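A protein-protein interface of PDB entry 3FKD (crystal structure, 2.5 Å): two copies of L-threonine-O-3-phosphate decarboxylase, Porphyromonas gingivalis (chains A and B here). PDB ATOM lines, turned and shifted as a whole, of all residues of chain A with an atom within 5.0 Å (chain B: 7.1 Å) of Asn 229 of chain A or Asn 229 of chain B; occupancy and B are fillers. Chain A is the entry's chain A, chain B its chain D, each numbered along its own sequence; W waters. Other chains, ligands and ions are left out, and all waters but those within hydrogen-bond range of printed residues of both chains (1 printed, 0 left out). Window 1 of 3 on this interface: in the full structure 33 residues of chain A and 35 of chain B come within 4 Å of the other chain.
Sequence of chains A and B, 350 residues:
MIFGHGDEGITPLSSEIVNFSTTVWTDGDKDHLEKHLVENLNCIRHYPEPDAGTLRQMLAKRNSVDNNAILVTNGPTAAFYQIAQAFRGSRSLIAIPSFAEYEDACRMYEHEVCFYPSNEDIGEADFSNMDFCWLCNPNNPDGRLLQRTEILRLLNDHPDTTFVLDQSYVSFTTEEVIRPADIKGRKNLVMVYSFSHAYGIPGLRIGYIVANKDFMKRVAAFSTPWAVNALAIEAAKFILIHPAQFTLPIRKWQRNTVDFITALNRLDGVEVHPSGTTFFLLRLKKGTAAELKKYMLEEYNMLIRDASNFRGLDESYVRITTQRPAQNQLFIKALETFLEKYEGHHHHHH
Of the 12 printed residues of chain A, 8 touch a printed residue of chain B. Of the 21 printed residues of chain B, 11 touch a printed residue of chain A. Among the printed residues, 16 pairs touch across the chains. Among the printed residues, no Asp or Glu carboxylate lies within 4 Å of a Lys or Arg side-chain nitrogen of the other chain.
Printed residues of chain B within 4 Å of Arg 205 of chain A: Pro 48 (3.98 Å), Trp 226 (2.7 Å) and Asn 229 (3.5 Å). Asn 229 of chain A touches just these residues of chain B: Gly 203 (3.5 Å), Leu 204 (3.9 Å), Arg 205 (3.4 Å) and Asn 229 (3.1 Å). Of the printed residues of chain B, Ala 230 of chain A touches Gly 203. Printed residues of chain B within 4 Å of Leu 231 of chain A: Leu 231 (3.1 Å). Of the printed residues of chain A, Arg 205 of chain B touches Asn 229 (3.4 Å). Val 228 of chain B touches none of the printed residues of chain A. Of the printed residues of chain A, Asn 229 of chain B touches Gly 203, Arg 205 and Asn 229. Ile 233 of chain B touches none of the printed residues of chain A. The nearest printed residue of chain A that does not touch Asn 229 of chain B is Leu 204 of chain A (4.01 Å). The nearest printed residue of chain B that does not touch Leu 231 of chain A is Leu 204 of chain B (4.1 Å).
The side-chain amide oxygen (OD1) of Asn 74 of chain A lies close to the backbone carbonyl oxygen (O) of Arg 205 of chain A (3.4 Å). The side-chain amide oxygen (OD1) of Asn 229 of chain B lies within hydrogen-bond range of the backbone NH (N) of Ala 232 of chain B (2.9 Å). The side-chain amide oxygen of Asn 74 of chain B sits close to the backbone carbonyl oxygen of Ala 227 of chain B (3.4 Å). The backbone NH (N) of Ala 232 of chain A sits at hydrogen-bond distance from the side-chain amide oxygen (OD1) of Asn 229 of chain A, 3.2 Å away. The side-chain amide nitrogen (ND2) of Asn 229 of chain B lies within hydrogen-bond range of the backbone carbonyl oxygen (O) of Leu 204 of chain B. The side-chain sulfur (SG) of Cys 43 of chain B lies within hydrogen-bond range of the backbone carbonyl oxygen (O) of Ala 230 of chain B (3.8 Å).
The guanidinium group (NE) of Arg 205 of chain A is in hydrogen-bond range of the backbone carbonyl oxygen (O) of Trp 226 of chain B, 2.7 Å away. ND2 of Asn 74 of chain A sits close to ND2 of Asn 74 of chain B, 3.2 Å away. O of Ala 227 of chain A is in hydrogen-bond range of ND2 of Asn 74 of chain B, 3.0 Å away. The backbone NH (N) of Ala 230 of chain B lies within hydrogen-bond range of the backbone carbonyl oxygen (O) of Gly 203 of chain A (3.0 Å). The side-chain amide nitrogen (ND2) of Asn 229 of chain A lies close to the side-chain amide nitrogen (ND2) of Asn 229 of chain B, 3.1 Å away. The backbone NH of Ala 230 of chain A sits at hydrogen-bond distance from the backbone carbonyl oxygen of Gly 203 of chain B (3.1 Å). The side-chain amide nitrogen (ND2) of Asn 74 of chain A sits at hydrogen-bond distance from the backbone carbonyl oxygen (O) of Ala 227 of chain B (2.9 Å). N of Gly 203 of chain A sits at hydrogen-bond distance from O of Ile 44 of chain B (3.1 Å).
Among the printed residues, pairs that only touch across the chains: Leu 231 of chain A with Leu 231 of chain B (3.1 Å), Asn 229 of chain A with Arg 205 of chain B (3.4 Å), Leu 204 of chain A with Ile 44 of chain B (3.4 Å), Asn 229 of chain A with Gly 203 of chain B (3.5 Å), Gly 203 of chain A with Asn 229 of chain B (3.5 Å), Arg 205 of chain A with Asn 229 of chain B (3.5 Å), Asn 229 of chain A with Leu 204 of chain B (3.9 Å) and Arg 205 of chain A with Pro 48 of chain B (3.98 Å).
Water W1 lies within hydrogen-bond range of ND2 of Asn 229 of chain A (2.9 Å), OD1 of Asn 74 of chain B (2.9 Å), OD1 of Asn 74 of chain A (2.9 Å) and ND2 of Asn 229 of chain B (3.0 Å).
Asn 74 of chain A touches Ala 227 of chain B, and with the chains exchanged Ala 227 of chain A touches Asn 74 of chain B. Gly 203 of chain A touches Asn 229 of chain B, and with the chains exchanged Asn 229 of chain A touches Gly 203 of chain B. Arg 205 of chain A touches Asn 229 of chain B, and with the chains exchanged Asn 229 of chain A touches Arg 205 of chain B. Leu 231 of chain A touches its own counterpart, Leu 231 of chain B. Of the 16 pairs that touch across the chains among the printed residues, 11 have their exchanged pair printed and touching as well.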
ATOM      1  N   PRO A  48     -17.571 -21.238   0.011  1.00  0.00           N
ATOM      2  CA  PRO A  48     -16.820 -21.786  -1.121  1.00  0.00           C
ATOM      3  C   PRO A  48     -17.798 -22.486  -2.045  1.00  0.00           C
ATOM      4  O   PRO A  48     -18.942 -22.752  -1.657  1.00  0.00           O
ATOM      5  CB  PRO A  48     -15.910 -22.834  -0.481  1.00  0.00           C
ATOM      6  CG  PRO A  48     -16.416 -23.023   0.915  1.00  0.00           C
ATOM      7  CD  PRO A  48     -17.610 -22.156   1.154  1.00  0.00           C
ATOM      8  N   ASN A  74     -11.986 -32.550   3.172  1.00  0.00           N
ATOM      9  CA  ASN A  74     -11.504 -31.719   4.267  1.00  0.00           C
ATOM     10  C   ASN A  74     -10.250 -32.325   4.928  1.00  0.00           C
ATOM     11  O   ASN A  74     -10.296 -32.648   6.100  1.00  0.00           O
ATOM     12  CB  ASN A  74     -12.595 -31.583   5.323  1.00  0.00           C
ATOM     13  CG  ASN A  74     -12.328 -30.494   6.359  1.00  0.00           C
ATOM     14  OD1 ASN A  74     -11.685 -29.516   6.104  1.00  0.00           O
ATOM     15  ND2 ASN A  74     -12.916 -30.663   7.545  1.00  0.00           N
ATOM     16  N   GLY A 203      -2.681 -27.281   8.674  1.00  0.00           N
ATOM     17  CA  GLY A 203      -3.742 -26.484   9.251  1.00  0.00           C
ATOM     18  C   GLY A 203      -4.859 -26.055   8.302  1.00  0.00           C
ATOM     19  O   GLY A 203      -5.923 -25.685   8.749  1.00  0.00           O
ATOM     20  N   LEU A 204      -4.619 -26.124   7.001  1.00  0.00           N
ATOM     21  CA  LEU A 204      -5.610 -25.799   6.006  1.00  0.00           C
ATOM     22  C   LEU A 204      -6.641 -26.890   5.789  1.00  0.00           C
ATOM     23  O   LEU A 204      -7.739 -26.609   5.320  1.00  0.00           O
ATOM     24  CB  LEU A 204      -4.934 -25.461   4.680  1.00  0.00           C
ATOM     25  CG  LEU A 204      -4.901 -24.007   4.222  1.00  0.00           C
ATOM     26  CD1 LEU A 204      -5.157 -23.115   5.407  1.00  0.00           C
ATOM     27  CD2 LEU A 204      -3.552 -23.671   3.558  1.00  0.00           C
ATOM     28  N   ARG A 205      -6.292 -28.124   6.140  1.00  0.00           N
ATOM     29  CA  ARG A 205      -7.198 -29.279   5.997  1.00  0.00           C
ATOM     30  C   ARG A 205      -7.691 -29.484   4.591  1.00  0.00           C
ATOM     31  O   ARG A 205      -8.835 -29.254   4.327  1.00  0.00           O
ATOM     32  CB  ARG A 205      -8.412 -29.162   6.927  1.00  0.00           C
ATOM     33  CG  ARG A 205      -8.069 -28.706   8.378  1.00  0.00           C
ATOM     34  CD  ARG A 205      -6.989 -29.573   9.132  1.00  0.00           C
ATOM     35  NE  ARG A 205      -7.328 -30.981   9.180  1.00  0.00           N
ATOM     36  CZ  ARG A 205      -6.616 -31.964   8.626  1.00  0.00           C
ATOM     37  NH1 ARG A 205      -5.476 -31.711   7.986  1.00  0.00           N
ATOM     38  NH2 ARG A 205      -7.036 -33.227   8.732  1.00  0.00           N
ATOM     39  N   ALA A 227     -17.922 -28.619   2.698  1.00  0.00           N
ATOM     40  CA  ALA A 227     -17.008 -29.372   3.576  1.00  0.00           C
ATOM     41  C   ALA A 227     -15.521 -28.959   3.437  1.00  0.00           C
ATOM     42  O   ALA A 227     -14.728 -29.190   4.366  1.00  0.00           O
ATOM     43  CB  ALA A 227     -17.150 -30.839   3.336  1.00  0.00           C
ATOM     44  N   VAL A 228     -15.175 -28.344   2.303  1.00  0.00           N
ATOM     45  CA  VAL A 228     -13.811 -27.860   2.053  1.00  0.00           C
ATOM     46  C   VAL A 228     -13.755 -26.334   2.106  1.00  0.00           C
ATOM     47  O   VAL A 228     -14.357 -25.661   1.264  1.00  0.00           O
ATOM     48  CB  VAL A 228     -13.260 -28.358   0.678  1.00  0.00           C
ATOM     49  CG1 VAL A 228     -11.848 -27.932   0.503  1.00  0.00           C
ATOM     50  CG2 VAL A 228     -13.364 -29.887   0.586  1.00  0.00           C
ATOM     51  N   ASN A 229     -13.039 -25.800   3.088  1.00  0.00           N
ATOM     52  CA  ASN A 229     -13.045 -24.371   3.313  1.00  0.00           C
ATOM     53  C   ASN A 229     -12.306 -23.565   2.212  1.00  0.00           C
ATOM     54  O   ASN A 229     -11.488 -24.114   1.452  1.00  0.00           O
ATOM     55  CB  ASN A 229     -12.528 -24.036   4.723  1.00  0.00           C
ATOM     56  CG  ASN A 229     -11.021 -24.279   4.877  1.00  0.00           C
ATOM     57  OD1 ASN A 229     -10.212 -23.449   4.461  1.00  0.00           O
ATOM     58  ND2 ASN A 229     -10.648 -25.445   5.442  1.00  0.00           N
ATOM     59  N   ALA A 230     -12.625 -22.268   2.158  1.00  0.00           N
ATOM     60  CA  ALA A 230     -12.329 -21.382   1.020  1.00  0.00           C
ATOM     61  C   ALA A 230     -10.870 -21.096   0.826  1.00  0.00           C
ATOM     62  O   ALA A 230     -10.387 -21.112  -0.290  1.00  0.00           O
ATOM     63  CB  ALA A 230     -13.118 -20.031   1.137  1.00  0.00           C
ATOM     64  N   LEU A 231     -10.177 -20.813   1.920  1.00  0.00           N
ATOM     65  CA  LEU A 231      -8.753 -20.535   1.879  1.00  0.00           C
ATOM     66  C   LEU A 231      -7.996 -21.761   1.451  1.00  0.00           C
ATOM     67  O   LEU A 231      -7.003 -21.628   0.749  1.00  0.00           O
ATOM     68  CB  LEU A 231      -8.243 -20.129   3.243  1.00  0.00           C
ATOM     69  CG  LEU A 231      -8.569 -18.713   3.669  1.00  0.00           C
ATOM     70  CD1 LEU A 231      -8.163 -18.585   5.137  1.00  0.00           C
ATOM     71  CD2 LEU A 231      -7.892 -17.635   2.749  1.00  0.00           C
ATOM     72  N   ALA A 232      -8.442 -22.939   1.891  1.00  0.00           N
ATOM     73  CA  ALA A 232      -7.793 -24.193   1.497  1.00  0.00           C
ATOM     74  C   ALA A 232      -7.916 -24.411   0.010  1.00  0.00           C
ATOM     75  O   ALA A 232      -6.958 -24.855  -0.636  1.00  0.00           O
ATOM     76  CB  ALA A 232      -8.342 -25.426   2.284  1.00  0.00           C
ATOM     77  N   ILE A 233      -9.087 -24.106  -0.538  1.00  0.00           N
ATOM     78  CA  ILE A 233      -9.328 -24.270  -1.972  1.00  0.00           C
ATOM     79  C   ILE A 233      -8.322 -23.384  -2.715  1.00  0.00           C
ATOM     80  O   ILE A 233      -7.741 -23.772  -3.729  1.00  0.00           O
ATOM     81  CB  ILE A 233     -10.831 -23.963  -2.382  1.00  0.00           C
ATOM     82  CG1 ILE A 233     -11.698 -25.233  -2.259  1.00  0.00           C
ATOM     83  CG2 ILE A 233     -10.919 -23.518  -3.798  1.00  0.00           C
ATOM     84  CD1 ILE A 233     -13.158 -24.987  -1.813  1.00  0.00           C
ATOM     85  N   CYS B  43      -0.291 -20.378  11.489  1.00  0.00           N
ATOM     86  CA  CYS B  43      -1.095 -21.449  12.058  1.00  0.00           C
ATOM     87  C   CYS B  43      -1.467 -22.503  11.030  1.00  0.00           C
ATOM     88  O   CYS B  43      -1.855 -23.582  11.383  1.00  0.00           O
ATOM     89  CB  CYS B  43      -2.343 -20.891  12.764  1.00  0.00           C
ATOM     90  SG  CYS B  43      -3.707 -20.448  11.691  1.00  0.00           S
ATOM     91  N   ILE B  44      -1.329 -22.191   9.747  1.00  0.00           N
ATOM     92  CA  ILE B  44      -1.648 -23.168   8.708  1.00  0.00           C
ATOM     93  C   ILE B  44      -0.517 -24.192   8.481  1.00  0.00           C
ATOM     94  O   ILE B  44      -0.671 -25.136   7.713  1.00  0.00           O
ATOM     95  CB  ILE B  44      -2.014 -22.495   7.379  1.00  0.00           C
ATOM     96  CG1 ILE B  44      -0.787 -21.905   6.697  1.00  0.00           C
ATOM     97  CG2 ILE B  44      -3.092 -21.450   7.591  1.00  0.00           C
ATOM     98  CD1 ILE B  44      -1.068 -21.492   5.218  1.00  0.00           C
ATOM     99  N   PRO B  48      -4.367 -28.267  13.733  1.00  0.00           N
ATOM    100  CA  PRO B  48      -5.200 -27.687  14.784  1.00  0.00           C
ATOM    101  C   PRO B  48      -5.293 -28.692  15.910  1.00  0.00           C
ATOM    102  O   PRO B  48      -5.066 -29.865  15.620  1.00  0.00           O
ATOM    103  CB  PRO B  48      -6.598 -27.603  14.144  1.00  0.00           C
ATOM    104  CG  PRO B  48      -6.514 -28.218  12.840  1.00  0.00           C
ATOM    105  CD  PRO B  48      -5.172 -28.885  12.676  1.00  0.00           C
ATOM    106  N   ALA B  52     -10.327 -29.048  18.537  1.00  0.00           N
ATOM    107  CA  ALA B  52     -10.563 -27.619  18.758  1.00  0.00           C
ATOM    108  C   ALA B  52     -10.843 -27.401  20.262  1.00  0.00           C
ATOM    109  O   ALA B  52     -11.718 -26.630  20.645  1.00  0.00           O
ATOM    110  CB  ALA B  52     -11.719 -27.138  17.882  1.00  0.00           C
ATOM    111  N   THR B  73     -17.530 -27.633  15.298  1.00  0.00           N
ATOM    112  CA  THR B  73     -17.879 -28.370  14.121  1.00  0.00           C
ATOM    113  C   THR B  73     -17.456 -27.635  12.847  1.00  0.00           C
ATOM    114  O   THR B  73     -17.325 -26.402  12.823  1.00  0.00           O
ATOM    115  CB  THR B  73     -19.380 -28.642  14.214  1.00  0.00           C
ATOM    116  OG1 THR B  73     -19.663 -30.039  13.992  1.00  0.00           O
ATOM    117  CG2 THR B  73     -20.175 -27.717  13.346  1.00  0.00           C
ATOM    118  N   ASN B  74     -17.226 -28.393  11.785  1.00  0.00           N
ATOM    119  CA  ASN B  74     -16.808 -27.822  10.506  1.00  0.00           C
ATOM    120  C   ASN B  74     -17.923 -27.036   9.877  1.00  0.00           C
ATOM    121  O   ASN B  74     -18.351 -27.346   8.771  1.00  0.00           O
ATOM    122  CB  ASN B  74     -16.377 -28.935   9.538  1.00  0.00           C
ATOM    123  CG  ASN B  74     -15.610 -28.407   8.330  1.00  0.00           C
ATOM    124  OD1 ASN B  74     -14.978 -27.378   8.397  1.00  0.00           O
ATOM    125  ND2 ASN B  74     -15.675 -29.123   7.228  1.00  0.00           N
ATOM    126  N   PRO B 202     -18.663 -17.008   6.226  1.00  0.00           N
ATOM    127  CA  PRO B 202     -19.065 -18.295   5.666  1.00  0.00           C
ATOM    128  C   PRO B 202     -17.901 -19.146   5.083  1.00  0.00           C
ATOM    129  O   PRO B 202     -18.033 -20.357   5.048  1.00  0.00           O
ATOM    130  CB  PRO B 202     -19.984 -17.863   4.535  1.00  0.00           C
ATOM    131  CG  PRO B 202     -19.518 -16.470   4.194  1.00  0.00           C
ATOM    132  CD  PRO B 202     -19.349 -15.907   5.531  1.00  0.00           C
ATOM    133  N   GLY B 203     -16.808 -18.534   4.616  1.00  0.00           N
ATOM    134  CA  GLY B 203     -15.727 -19.267   3.964  1.00  0.00           C
ATOM    135  C   GLY B 203     -14.822 -20.045   4.911  1.00  0.00           C
ATOM    136  O   GLY B 203     -14.094 -20.948   4.511  1.00  0.00           O
ATOM    137  N   LEU B 204     -14.884 -19.700   6.183  1.00  0.00           N
ATOM    138  CA  LEU B 204     -14.075 -20.346   7.216  1.00  0.00           C
ATOM    139  C   LEU B 204     -14.601 -21.728   7.710  1.00  0.00           C
ATOM    140  O   LEU B 204     -13.843 -22.559   8.141  1.00  0.00           O
ATOM    141  CB  LEU B 204     -13.874 -19.374   8.386  1.00  0.00           C
ATOM    142  CG  LEU B 204     -12.532 -18.650   8.560  1.00  0.00           C
ATOM    143  CD1 LEU B 204     -11.589 -18.757   7.367  1.00  0.00           C
ATOM    144  CD2 LEU B 204     -12.757 -17.228   8.975  1.00  0.00           C
ATOM    145  N   ARG B 205     -15.896 -21.971   7.590  1.00  0.00           N
ATOM    146  CA  ARG B 205     -16.509 -23.235   8.019  1.00  0.00           C
ATOM    147  C   ARG B 205     -16.319 -23.570   9.503  1.00  0.00           C
ATOM    148  O   ARG B 205     -15.590 -24.492   9.838  1.00  0.00           O
ATOM    149  CB  ARG B 205     -16.006 -24.376   7.140  1.00  0.00           C
ATOM    150  CG  ARG B 205     -15.802 -23.974   5.668  1.00  0.00           C
ATOM    151  CD  ARG B 205     -17.066 -23.419   4.958  1.00  0.00           C
ATOM    152  NE  ARG B 205     -18.218 -24.312   5.185  1.00  0.00           N
ATOM    153  CZ  ARG B 205     -19.373 -23.963   5.751  1.00  0.00           C
ATOM    154  NH1 ARG B 205     -19.597 -22.696   6.123  1.00  0.00           N
ATOM    155  NH2 ARG B 205     -20.321 -24.899   5.924  1.00  0.00           N
ATOM    156  N   ILE B 206     -16.973 -22.827  10.390  1.00  0.00           N
ATOM    157  CA  ILE B 206     -17.028 -23.192  11.808  1.00  0.00           C
ATOM    158  C   ILE B 206     -18.403 -22.968  12.448  1.00  0.00           C
ATOM    159  O   ILE B 206     -19.036 -21.927  12.248  1.00  0.00           O
ATOM    160  CB  ILE B 206     -16.181 -22.295  12.692  1.00  0.00           C
ATOM    161  CG1 ILE B 206     -15.416 -21.270  11.883  1.00  0.00           C
ATOM    162  CG2 ILE B 206     -15.408 -23.098  13.695  1.00  0.00           C
ATOM    163  CD1 ILE B 206     -15.207 -20.037  12.674  1.00  0.00           C
ATOM    164  N   TRP B 226      -9.262 -33.205  13.632  1.00  0.00           N
ATOM    165  CA  TRP B 226      -8.819 -32.144  12.722  1.00  0.00           C
ATOM    166  C   TRP B 226      -9.881 -31.808  11.697  1.00  0.00           C
ATOM    167  O   TRP B 226      -9.553 -31.497  10.572  1.00  0.00           O
ATOM    168  CB  TRP B 226      -7.564 -32.553  11.951  1.00  0.00           C
ATOM    169  CG  TRP B 226      -6.465 -33.124  12.795  1.00  0.00           C
ATOM    170  CD1 TRP B 226      -5.823 -32.510  13.819  1.00  0.00           C
ATOM    171  CD2 TRP B 226      -5.876 -34.430  12.675  1.00  0.00           C
ATOM    172  NE1 TRP B 226      -4.890 -33.344  14.354  1.00  0.00           N
ATOM    173  CE2 TRP B 226      -4.890 -34.529  13.666  1.00  0.00           C
ATOM    174  CE3 TRP B 226      -6.105 -35.533  11.834  1.00  0.00           C
ATOM    175  CZ2 TRP B 226      -4.118 -35.689  13.854  1.00  0.00           C
ATOM    176  CZ3 TRP B 226      -5.322 -36.692  12.009  1.00  0.00           C
ATOM    177  CH2 TRP B 226      -4.336 -36.747  13.010  1.00  0.00           C
ATOM    178  N   ALA B 227     -11.149 -31.915  12.091  1.00  0.00           N
ATOM    179  CA  ALA B 227     -12.278 -31.582  11.245  1.00  0.00           C
ATOM    180  C   ALA B 227     -12.451 -30.060  11.155  1.00  0.00           C
ATOM    181  O   ALA B 227     -13.059 -29.544  10.218  1.00  0.00           O
ATOM    182  CB  ALA B 227     -13.567 -32.249  11.791  1.00  0.00           C
ATOM    183  N   VAL B 228     -11.915 -29.347  12.136  1.00  0.00           N
ATOM    184  CA  VAL B 228     -12.027 -27.903  12.139  1.00  0.00           C
ATOM    185  C   VAL B 228     -10.684 -27.289  11.802  1.00  0.00           C
ATOM    186  O   VAL B 228      -9.765 -27.484  12.540  1.00  0.00           O
ATOM    187  CB  VAL B 228     -12.489 -27.380  13.506  1.00  0.00           C
ATOM    188  CG1 VAL B 228     -12.855 -25.880  13.417  1.00  0.00           C
ATOM    189  CG2 VAL B 228     -13.676 -28.274  14.047  1.00  0.00           C
ATOM    190  N   ASN B 229     -10.596 -26.545  10.698  1.00  0.00           N
ATOM    191  CA  ASN B 229      -9.341 -25.953  10.223  1.00  0.00           C
ATOM    192  C   ASN B 229      -8.770 -24.864  11.142  1.00  0.00           C
ATOM    193  O   ASN B 229      -9.516 -24.198  11.849  1.00  0.00           O
ATOM    194  CB  ASN B 229      -9.450 -25.465   8.761  1.00  0.00           C
ATOM    195  CG  ASN B 229     -10.255 -24.192   8.630  1.00  0.00           C
ATOM    196  OD1 ASN B 229      -9.763 -23.109   8.915  1.00  0.00           O
ATOM    197  ND2 ASN B 229     -11.513 -24.315   8.200  1.00  0.00           N
ATOM    198  N   ALA B 230      -7.439 -24.728  11.131  1.00  0.00           N
ATOM    199  CA  ALA B 230      -6.729 -23.793  12.029  1.00  0.00           C
ATOM    200  C   ALA B 230      -7.062 -22.280  11.926  1.00  0.00           C
ATOM    201  O   ALA B 230      -7.066 -21.581  12.940  1.00  0.00           O
ATOM    202  CB  ALA B 230      -5.250 -24.001  11.932  1.00  0.00           C
ATOM    203  N   LEU B 231      -7.309 -21.771  10.720  1.00  0.00           N
ATOM    204  CA  LEU B 231      -7.727 -20.366  10.560  1.00  0.00           C
ATOM    205  C   LEU B 231      -9.090 -20.094  11.192  1.00  0.00           C
ATOM    206  O   LEU B 231      -9.249 -19.127  11.941  1.00  0.00           O
ATOM    207  CB  LEU B 231      -7.709 -19.947   9.105  1.00  0.00           C
ATOM    208  CG  LEU B 231      -6.269 -19.603   8.752  1.00  0.00           C
ATOM    209  CD1 LEU B 231      -6.041 -19.481   7.244  1.00  0.00           C
ATOM    210  CD2 LEU B 231      -5.766 -18.344   9.516  1.00  0.00           C
ATOM    211  N   ALA B 232     -10.050 -20.987  10.919  1.00  0.00           N
ATOM    212  CA  ALA B 232     -11.374 -20.910  11.501  1.00  0.00           C
ATOM    213  C   ALA B 232     -11.329 -20.845  13.037  1.00  0.00           C
ATOM    214  O   ALA B 232     -12.022 -20.030  13.646  1.00  0.00           O
ATOM    215  CB  ALA B 232     -12.204 -22.068  11.036  1.00  0.00           C
ATOM    216  N   ILE B 233     -10.513 -21.694  13.662  1.00  0.00           N
ATOM    217  CA  ILE B 233     -10.363 -21.688  15.119  1.00  0.00           C
ATOM    218  C   ILE B 233      -9.737 -20.369  15.604  1.00  0.00           C
ATOM    219  O   ILE B 233     -10.232 -19.750  16.547  1.00  0.00           O
ATOM    220  CB  ILE B 233      -9.535 -22.893  15.625  1.00  0.00           C
ATOM    221  CG1 ILE B 233     -10.293 -24.216  15.490  1.00  0.00           C
ATOM    222  CG2 ILE B 233      -9.050 -22.684  17.063  1.00  0.00           C
ATOM    223  CD1 ILE B 233      -9.344 -25.504  15.643  1.00  0.00           C
ATOM    224  N   GLU B 234      -8.641 -19.956  14.963  1.00  0.00           N
ATOM    225  CA  GLU B 234      -8.005 -18.673  15.224  1.00  0.00           C
ATOM    226  C   GLU B 234      -8.989 -17.503  15.072  1.00  0.00           C
ATOM    227  O   GLU B 234      -9.003 -16.595  15.882  1.00  0.00           O
ATOM    228  CB  GLU B 234      -6.800 -18.481  14.291  1.00  0.00           C
ATOM    229  CG  GLU B 234      -5.977 -17.262  14.576  1.00  0.00           C
ATOM    230  CD  GLU B 234      -5.301 -17.325  15.943  1.00  0.00           C
ATOM    231  OE1 GLU B 234      -4.869 -18.420  16.371  1.00  0.00           O
ATOM    232  OE2 GLU B 234      -5.202 -16.268  16.592  1.00  0.00           O
ATOM    233  N   ALA B 235      -9.810 -17.536  14.035  1.00  0.00           N
ATOM    234  CA  ALA B 235     -10.798 -16.491  13.819  1.00  0.00           C
ATOM    235  C   ALA B 235     -11.858 -16.502  14.925  1.00  0.00           C
ATOM    236  O   ALA B 235     -12.205 -15.455  15.469  1.00  0.00           O
ATOM    237  CB  ALA B 235     -11.449 -16.632  12.436  1.00  0.00           C
HETATM  238  O   HOH W   1     -12.462 -26.896   7.096  1.00  0.00           O
